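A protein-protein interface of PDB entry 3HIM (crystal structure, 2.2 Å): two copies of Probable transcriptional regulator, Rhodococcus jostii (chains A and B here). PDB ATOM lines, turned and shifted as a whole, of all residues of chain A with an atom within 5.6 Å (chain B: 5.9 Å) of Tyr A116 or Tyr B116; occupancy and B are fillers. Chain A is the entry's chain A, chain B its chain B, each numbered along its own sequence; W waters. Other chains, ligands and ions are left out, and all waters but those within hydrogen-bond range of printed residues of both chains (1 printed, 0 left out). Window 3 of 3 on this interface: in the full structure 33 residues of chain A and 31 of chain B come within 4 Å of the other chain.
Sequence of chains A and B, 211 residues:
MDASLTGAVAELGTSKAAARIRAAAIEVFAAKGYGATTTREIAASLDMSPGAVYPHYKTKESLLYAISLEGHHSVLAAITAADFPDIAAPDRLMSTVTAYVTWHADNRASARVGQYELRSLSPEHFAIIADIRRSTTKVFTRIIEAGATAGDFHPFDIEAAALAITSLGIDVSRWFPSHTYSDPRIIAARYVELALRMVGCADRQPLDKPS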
ATOM      1  N   ALA A 111      16.432  29.584 -20.956  1.00  0.00           N
ATOM      2  CA  ALA A 111      16.981  29.052 -19.710  1.00  0.00           C
ATOM      3  C   ALA A 111      15.909  28.546 -18.737  1.00  0.00           C
ATOM      4  O   ALA A 111      16.073  27.503 -18.093  1.00  0.00           O
ATOM      5  CB  ALA A 111      17.893  30.091 -19.030  1.00  0.00           C
ATOM      6  N   ARG A 112      14.830  29.308 -18.616  1.00  0.00           N
ATOM      7  CA  ARG A 112      13.728  28.965 -17.725  1.00  0.00           C
ATOM      8  C   ARG A 112      13.161  27.614 -18.134  1.00  0.00           C
ATOM      9  O   ARG A 112      12.983  26.735 -17.297  1.00  0.00           O
ATOM     10  CB  ARG A 112      12.624  30.024 -17.810  1.00  0.00           C
ATOM     11  CG  ARG A 112      12.643  31.067 -16.704  1.00  0.00           C
ATOM     12  CD  ARG A 112      11.369  31.913 -16.762  1.00  0.00           C
ATOM     13  NE  ARG A 112      11.433  32.964 -17.777  1.00  0.00           N
ATOM     14  CZ  ARG A 112      11.520  34.276 -17.527  1.00  0.00           C
ATOM     15  NH1 ARG A 112      11.544  34.745 -16.281  1.00  0.00           N
ATOM     16  NH2 ARG A 112      11.571  35.136 -18.541  1.00  0.00           N
ATOM     17  N   VAL A 113      12.897  27.455 -19.432  1.00  0.00           N
ATOM     18  CA  VAL A 113      12.344  26.213 -19.956  1.00  0.00           C
ATOM     19  C   VAL A 113      13.350  25.076 -19.779  1.00  0.00           C
ATOM     20  O   VAL A 113      12.996  24.030 -19.234  1.00  0.00           O
ATOM     21  CB  VAL A 113      11.914  26.344 -21.431  1.00  0.00           C
ATOM     22  CG1 VAL A 113      11.439  25.000 -21.982  1.00  0.00           C
ATOM     23  CG2 VAL A 113      10.825  27.419 -21.577  1.00  0.00           C
ATOM     24  N   GLY A 114      14.596  25.300 -20.197  1.00  0.00           N
ATOM     25  CA  GLY A 114      15.633  24.273 -20.147  1.00  0.00           C
ATOM     26  C   GLY A 114      16.099  23.881 -18.752  1.00  0.00           C
ATOM     27  O   GLY A 114      16.757  22.850 -18.579  1.00  0.00           O
ATOM     28  N   GLN A 115      15.758  24.688 -17.753  1.00  0.00           N
ATOM     29  CA  GLN A 115      16.286  24.496 -16.410  1.00  0.00           C
ATOM     30  C   GLN A 115      15.232  24.176 -15.349  1.00  0.00           C
ATOM     31  O   GLN A 115      15.556  23.547 -14.346  1.00  0.00           O
ATOM     32  CB  GLN A 115      17.057  25.752 -16.001  1.00  0.00           C
ATOM     33  CG  GLN A 115      18.292  25.497 -15.187  1.00  0.00           C
ATOM     34  CD  GLN A 115      19.478  24.985 -15.987  1.00  0.00           C
ATOM     35  OE1 GLN A 115      20.036  25.689 -16.843  1.00  0.00           O
ATOM     36  NE2 GLN A 115      19.915  23.771 -15.660  1.00  0.00           N
ATOM     37  N   TYR A 116      13.987  24.622 -15.561  1.00  0.00           N
ATOM     38  CA  TYR A 116      12.937  24.534 -14.547  1.00  0.00           C
ATOM     39  C   TYR A 116      11.956  23.378 -14.734  1.00  0.00           C
ATOM     40  O   TYR A 116      11.003  23.227 -13.958  1.00  0.00           O
ATOM     41  CB  TYR A 116      12.195  25.870 -14.428  1.00  0.00           C
ATOM     42  CG  TYR A 116      13.023  26.899 -13.685  1.00  0.00           C
ATOM     43  CD1 TYR A 116      14.077  27.554 -14.321  1.00  0.00           C
ATOM     44  CD2 TYR A 116      12.779  27.190 -12.334  1.00  0.00           C
ATOM     45  CE1 TYR A 116      14.869  28.479 -13.632  1.00  0.00           C
ATOM     46  CE2 TYR A 116      13.557  28.113 -11.649  1.00  0.00           C
ATOM     47  CZ  TYR A 116      14.600  28.751 -12.306  1.00  0.00           C
ATOM     48  OH  TYR A 116      15.399  29.657 -11.663  1.00  0.00           O
ATOM     49  N   GLU A 117      12.202  22.568 -15.763  1.00  0.00           N
ATOM     50  CA  GLU A 117      11.339  21.446 -16.093  1.00  0.00           C
ATOM     51  C   GLU A 117      12.110  20.145 -16.184  1.00  0.00           C
ATOM     52  O   GLU A 117      11.602  19.183 -16.755  1.00  0.00           O
ATOM     53  CB  GLU A 117      10.631  21.678 -17.434  1.00  0.00           C
ATOM     54  CG  GLU A 117       9.963  23.019 -17.604  1.00  0.00           C
ATOM     55  CD  GLU A 117       8.643  23.168 -16.853  1.00  0.00           C
ATOM     56  OE1 GLU A 117       8.117  22.182 -16.283  1.00  0.00           O
ATOM     57  OE2 GLU A 117       8.112  24.293 -16.859  1.00  0.00           O
ATOM     58  N   LEU A 118      13.323  20.097 -15.635  1.00  0.00           N
ATOM     59  CA  LEU A 118      14.157  18.901 -15.781  1.00  0.00           C
ATOM     60  C   LEU A 118      13.469  17.620 -15.293  1.00  0.00           C
ATOM     61  O   LEU A 118      13.768  16.528 -15.782  1.00  0.00           O
ATOM     62  CB  LEU A 118      15.510  19.066 -15.083  1.00  0.00           C
ATOM     63  CG  LEU A 118      16.491  20.102 -15.661  1.00  0.00           C
ATOM     64  CD1 LEU A 118      17.527  20.495 -14.594  1.00  0.00           C
ATOM     65  CD2 LEU A 118      17.160  19.605 -16.945  1.00  0.00           C
ATOM     66  N   ILE A 170      21.872  30.590 -12.890  1.00  0.00           N
ATOM     67  CA  ILE A 170      20.652  30.002 -13.415  1.00  0.00           C
ATOM     68  C   ILE A 170      19.469  30.807 -12.885  1.00  0.00           C
ATOM     69  O   ILE A 170      18.563  31.153 -13.641  1.00  0.00           O
ATOM     70  CB  ILE A 170      20.527  28.517 -13.040  1.00  0.00           C
ATOM     71  CG1 ILE A 170      21.504  27.696 -13.893  1.00  0.00           C
ATOM     72  CG2 ILE A 170      19.077  28.017 -13.265  1.00  0.00           C
ATOM     73  CD1 ILE A 170      21.748  26.290 -13.393  1.00  0.00           C
ATOM     74  N   ASP A 171      19.515  31.142 -11.596  1.00  0.00           N
ATOM     75  CA  ASP A 171      18.391  31.817 -10.954  1.00  0.00           C
ATOM     76  C   ASP A 171      18.105  33.218 -11.506  1.00  0.00           C
ATOM     77  O   ASP A 171      16.970  33.709 -11.432  1.00  0.00           O
ATOM     78  CB  ASP A 171      18.547  31.845  -9.427  1.00  0.00           C
ATOM     79  CG  ASP A 171      17.270  32.238  -8.736  1.00  0.00           C
ATOM     80  OD1 ASP A 171      16.233  31.564  -8.954  1.00  0.00           O
ATOM     81  OD2 ASP A 171      17.290  33.238  -7.993  1.00  0.00           O
ATOM     82  N   SER A 173      17.707  33.889 -14.512  1.00  0.00           N
ATOM     83  CA  SER A 173      16.685  33.720 -15.533  1.00  0.00           C
ATOM     84  C   SER A 173      15.272  33.756 -14.934  1.00  0.00           C
ATOM     85  O   SER A 173      14.314  34.125 -15.607  1.00  0.00           O
ATOM     86  CB  SER A 173      16.938  32.442 -16.333  1.00  0.00           C
ATOM     87  OG  SER A 173      18.165  32.544 -17.036  1.00  0.00           O
ATOM     88  N   ARG A 174      15.157  33.404 -13.658  1.00  0.00           N
ATOM     89  CA  ARG A 174      13.877  33.505 -12.959  1.00  0.00           C
ATOM     90  C   ARG A 174      13.510  34.970 -12.657  1.00  0.00           C
ATOM     91  O   ARG A 174      12.423  35.426 -13.047  1.00  0.00           O
ATOM     92  CB  ARG A 174      13.850  32.660 -11.679  1.00  0.00           C
ATOM     93  CG  ARG A 174      12.529  32.807 -10.895  1.00  0.00           C
ATOM     94  CD  ARG A 174      12.587  32.173  -9.517  1.00  0.00           C
ATOM     95  NE  ARG A 174      13.681  32.723  -8.717  1.00  0.00           N
ATOM     96  CZ  ARG A 174      13.587  33.801  -7.939  1.00  0.00           C
ATOM     97  NH1 ARG A 174      12.441  34.472  -7.846  1.00  0.00           N
ATOM     98  NH2 ARG A 174      14.644  34.227  -7.265  1.00  0.00           N
ATOM     99  N   ALA B 111       7.229  24.822  -2.557  1.00  0.00           N
ATOM    100  CA  ALA B 111       7.980  26.036  -2.953  1.00  0.00           C
ATOM    101  C   ALA B 111       7.896  26.267  -4.464  1.00  0.00           C
ATOM    102  O   ALA B 111       7.629  27.385  -4.904  1.00  0.00           O
ATOM    103  CB  ALA B 111       9.423  25.955  -2.507  1.00  0.00           C
ATOM    104  N   ARG B 112       8.103  25.210  -5.248  1.00  0.00           N
ATOM    105  CA  ARG B 112       8.001  25.317  -6.698  1.00  0.00           C
ATOM    106  C   ARG B 112       6.638  25.848  -7.174  1.00  0.00           C
ATOM    107  O   ARG B 112       6.577  26.745  -8.014  1.00  0.00           O
ATOM    108  CB  ARG B 112       8.333  23.975  -7.350  1.00  0.00           C
ATOM    109  CG  ARG B 112       9.833  23.718  -7.396  1.00  0.00           C
ATOM    110  CD  ARG B 112      10.192  22.422  -8.096  1.00  0.00           C
ATOM    111  NE  ARG B 112      10.506  21.374  -7.125  1.00  0.00           N
ATOM    112  CZ  ARG B 112       9.837  20.234  -7.017  1.00  0.00           C
ATOM    113  NH1 ARG B 112       8.823  19.987  -7.841  1.00  0.00           N
ATOM    114  NH2 ARG B 112      10.187  19.333  -6.099  1.00  0.00           N
ATOM    115  N   VAL B 113       5.556  25.303  -6.621  1.00  0.00           N
ATOM    116  CA  VAL B 113       4.206  25.688  -7.034  1.00  0.00           C
ATOM    117  C   VAL B 113       3.960  27.162  -6.668  1.00  0.00           C
ATOM    118  O   VAL B 113       3.483  27.949  -7.491  1.00  0.00           O
ATOM    119  CB  VAL B 113       3.113  24.737  -6.440  1.00  0.00           C
ATOM    120  CG1 VAL B 113       1.726  25.293  -6.673  1.00  0.00           C
ATOM    121  CG2 VAL B 113       3.230  23.317  -7.052  1.00  0.00           C
ATOM    122  N   GLY B 114       4.335  27.517  -5.443  1.00  0.00           N
ATOM    123  CA  GLY B 114       4.296  28.892  -4.980  1.00  0.00           C
ATOM    124  C   GLY B 114       5.097  29.860  -5.823  1.00  0.00           C
ATOM    125  O   GLY B 114       4.623  30.944  -6.102  1.00  0.00           O
ATOM    126  N   GLN B 115       6.313  29.478  -6.217  1.00  0.00           N
ATOM    127  CA  GLN B 115       7.202  30.385  -6.946  1.00  0.00           C
ATOM    128  C   GLN B 115       6.911  30.476  -8.456  1.00  0.00           C
ATOM    129  O   GLN B 115       6.922  31.557  -9.017  1.00  0.00           O
ATOM    130  CB  GLN B 115       8.676  30.019  -6.716  1.00  0.00           C
ATOM    131  N   TYR B 116       6.640  29.345  -9.104  1.00  0.00           N
ATOM    132  CA  TYR B 116       6.699  29.295 -10.563  1.00  0.00           C
ATOM    133  C   TYR B 116       5.392  29.722 -11.223  1.00  0.00           C
ATOM    134  O   TYR B 116       5.374  30.049 -12.412  1.00  0.00           O
ATOM    135  CB  TYR B 116       7.123  27.905 -11.076  1.00  0.00           C
ATOM    136  CG  TYR B 116       8.466  27.350 -10.580  1.00  0.00           C
ATOM    137  CD1 TYR B 116       9.357  28.127  -9.832  1.00  0.00           C
ATOM    138  CD2 TYR B 116       8.846  26.041 -10.891  1.00  0.00           C
ATOM    139  CE1 TYR B 116      10.574  27.607  -9.383  1.00  0.00           C
ATOM    140  CE2 TYR B 116      10.065  25.513 -10.459  1.00  0.00           C
ATOM    141  CZ  TYR B 116      10.917  26.298  -9.694  1.00  0.00           C
ATOM    142  OH  TYR B 116      12.124  25.773  -9.268  1.00  0.00           O
ATOM    143  N   GLU B 117       4.305  29.732 -10.456  1.00  0.00           N
ATOM    144  CA  GLU B 117       3.005  30.116 -11.008  1.00  0.00           C
ATOM    145  C   GLU B 117       2.495  31.500 -10.537  1.00  0.00           C
ATOM    146  O   GLU B 117       1.288  31.743 -10.528  1.00  0.00           O
ATOM    147  CB  GLU B 117       1.961  29.023 -10.738  1.00  0.00           C
ATOM    148  CG  GLU B 117       2.452  27.604 -10.950  1.00  0.00           C
ATOM    149  CD  GLU B 117       2.438  27.148 -12.407  1.00  0.00           C
ATOM    150  OE1 GLU B 117       2.192  27.976 -13.318  1.00  0.00           O
ATOM    151  OE2 GLU B 117       2.659  25.929 -12.641  1.00  0.00           O
ATOM    152  N   LEU B 118       3.408  32.399 -10.167  1.00  0.00           N
ATOM    153  CA  LEU B 118       3.036  33.745  -9.697  1.00  0.00           C
ATOM    154  C   LEU B 118       2.290  34.560 -10.736  1.00  0.00           C
ATOM    155  O   LEU B 118       1.442  35.394 -10.389  1.00  0.00           O
ATOM    156  CB  LEU B 118       4.258  34.537  -9.252  1.00  0.00           C
ATOM    157  CG  LEU B 118       4.939  34.056  -7.972  1.00  0.00           C
ATOM    158  CD1 LEU B 118       6.356  34.622  -7.917  1.00  0.00           C
ATOM    159  CD2 LEU B 118       4.129  34.441  -6.732  1.00  0.00           C
ATOM    160  N   ARG B 119       2.617  34.295 -11.994  1.00  0.00           N
ATOM    161  CA  ARG B 119       1.977  34.909 -13.152  1.00  0.00           C
ATOM    162  C   ARG B 119       0.484  34.607 -13.188  1.00  0.00           C
ATOM    163  O   ARG B 119      -0.271  35.313 -13.864  1.00  0.00           O
ATOM    164  CB  ARG B 119       2.618  34.392 -14.451  1.00  0.00           C
ATOM    165  CG  ARG B 119       2.363  32.901 -14.682  1.00  0.00           C
ATOM    166  CD  ARG B 119       2.991  32.344 -15.947  1.00  0.00           C
ATOM    167  NE  ARG B 119       2.998  30.886 -15.867  1.00  0.00           N
ATOM    168  CZ  ARG B 119       4.070  30.121 -16.013  1.00  0.00           C
ATOM    169  NH1 ARG B 119       5.249  30.651 -16.299  1.00  0.00           N
ATOM    170  NH2 ARG B 119       3.957  28.810 -15.898  1.00  0.00           N
ATOM    171  N   ILE B 170      16.127  29.815  -2.665  1.00  0.00           N
ATOM    172  CA  ILE B 170      15.036  29.567  -3.582  1.00  0.00           C
ATOM    173  C   ILE B 170      15.407  28.549  -4.660  1.00  0.00           C
ATOM    174  O   ILE B 170      14.582  27.711  -5.016  1.00  0.00           O
ATOM    175  CB  ILE B 170      14.577  30.874  -4.247  1.00  0.00           C
ATOM    176  CG1 ILE B 170      13.817  31.737  -3.229  1.00  0.00           C
ATOM    177  CG2 ILE B 170      13.725  30.571  -5.500  1.00  0.00           C
ATOM    178  CD1 ILE B 170      13.709  33.226  -3.626  1.00  0.00           C
ATOM    179  N   ASP B 171      16.643  28.606  -5.168  1.00  0.00           N
ATOM    180  CA  ASP B 171      17.031  27.693  -6.241  1.00  0.00           C
ATOM    181  C   ASP B 171      17.235  26.258  -5.755  1.00  0.00           C
ATOM    182  O   ASP B 171      17.108  25.319  -6.521  1.00  0.00           O
ATOM    183  CB  ASP B 171      18.264  28.185  -6.992  1.00  0.00           C
ATOM    184  CG  ASP B 171      18.463  27.458  -8.313  1.00  0.00           C
ATOM    185  OD1 ASP B 171      17.618  27.596  -9.240  1.00  0.00           O
ATOM    186  OD2 ASP B 171      19.475  26.744  -8.428  1.00  0.00           O
ATOM    187  N   SER B 173      15.155  24.729  -4.177  1.00  0.00           N
ATOM    188  CA  SER B 173      13.875  24.043  -4.401  1.00  0.00           C
ATOM    189  C   SER B 173      13.772  23.468  -5.816  1.00  0.00           C
ATOM    190  O   SER B 173      12.986  22.558  -6.062  1.00  0.00           O
ATOM    191  CB  SER B 173      12.676  24.946  -4.087  1.00  0.00           C
ATOM    192  OG  SER B 173      12.668  25.290  -2.714  1.00  0.00           O
ATOM    193  N   ARG B 174      14.576  24.005  -6.732  1.00  0.00           N
ATOM    194  CA  ARG B 174      14.636  23.517  -8.107  1.00  0.00           C
ATOM    195  C   ARG B 174      15.470  22.253  -8.217  1.00  0.00           C
ATOM    196  O   ARG B 174      14.986  21.264  -8.737  1.00  0.00           O
ATOM    197  CB  ARG B 174      15.207  24.586  -9.052  1.00  0.00           C
ATOM    198  CG  ARG B 174      15.199  24.190 -10.550  1.00  0.00           C
ATOM    199  CD  ARG B 174      15.900  25.257 -11.430  1.00  0.00           C
ATOM    200  NE  ARG B 174      17.268  25.482 -10.955  1.00  0.00           N
ATOM    201  CZ  ARG B 174      18.291  24.673 -11.197  1.00  0.00           C
ATOM    202  NH1 ARG B 174      18.140  23.587 -11.964  1.00  0.00           N
ATOM    203  NH2 ARG B 174      19.476  24.951 -10.683  1.00  0.00           N
HETATM  204  O   HOH W   1      15.446  29.209  -9.153  1.00  0.00           O
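O of Arg A174 is in hydrogen-bond range of NH1 of Arg A112 (3.4 Å).
The guanidinium group (NE) of Arg A174 lies within salt-bridge range of the side-chain carboxylate (OD1) of Asp A171, 2.8 Å away.
OD1 of Asp B171 lies within salt-bridge range of NE of Arg B174, at 2.7 Å.
The side-chain hydroxyl (OH) of Tyr A116 sits at hydrogen-bond distance from the side-chain carboxylate (OD1) of Asp A171, 3.4 Å away.
O of Gln A115 touches CD of Arg B174 (3.4 Å).
CD2 of Tyr A116 touches CZ of Tyr B116 (3.4 Å).
Asp B171 touches Tyr A116.
Tyr A116 touches Arg B174 (CE2 to CD, 3.7 Å).
Arg B174 touches Ile A170 (NH2 to CD1, 3.8 Å).
Arg A174 touches Ile B170.
Of the printed residues of chain B, Gln A115 touches Arg B174 (3.4 Å).
Tyr A116 touches just these residues of chain B: Tyr B116 (3.4 Å), Asp B171 (3.9 Å) and Arg B174 (3.7 Å).
Of the printed residues of chain B, Arg A174 touches Ile B170 (3.9 Å).
Of chain A, only Tyr A116 comes within 4 Å of Tyr B116.
Printed residues of chain A within 4 Å of Arg B174: Gln A115 (3.4 Å), Tyr A116 (3.7 Å) and Ile A170 (3.8 Å).
The nearest printed residue of chain B that does not touch Tyr A116 is Arg B112 (6.0 Å).
The nearest residue of chain A that does not touch Tyr B116 is Arg A174 (5.0 Å).
Of the 12 printed residues of chain A, 4 touch a printed residue of chain B.
Hydrophobic or aromatic side chains of chain A that line the printed part of chain B: Tyr A116 and Ile A170.
Along chain A the printed residues that touch a printed residue of chain B span positions 115 to 174.
Printed residues of chain B that touch a printed residue of chain A: Tyr B116, Ile B170, Asp B171 and Arg B174.
Among the printed residues, 6 pairs touch across the chains.
Among the printed residues, no Asp or Glu carboxylate lies within 4 Å of a Lys or Arg side-chain nitrogen of the other chain.
Gln A115 touches Arg B174, but with the chains exchanged Arg A174 does not touch Gln B115 (5.3 Å).
Tyr B116 touches its own counterpart, Tyr A116.
Tyr A116 touches Arg B174, but with the chains exchanged Arg A174 does not touch Tyr B116 (5.0 Å).
Ile A170 touches Arg B174, and with the chains exchanged Arg A174 touches Ile B170.
12 positions are printed for both chains.
Of the 6 pairs that touch across the chains among the printed residues, 3 have their exchanged pair printed and touching as well.
Water W1 lies within hydrogen-bond range of OD1 of Asp A171 (2.5 Å), OH of Tyr A116 (2.6 Å) and OD1 of Asp B171 (2.7 Å).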
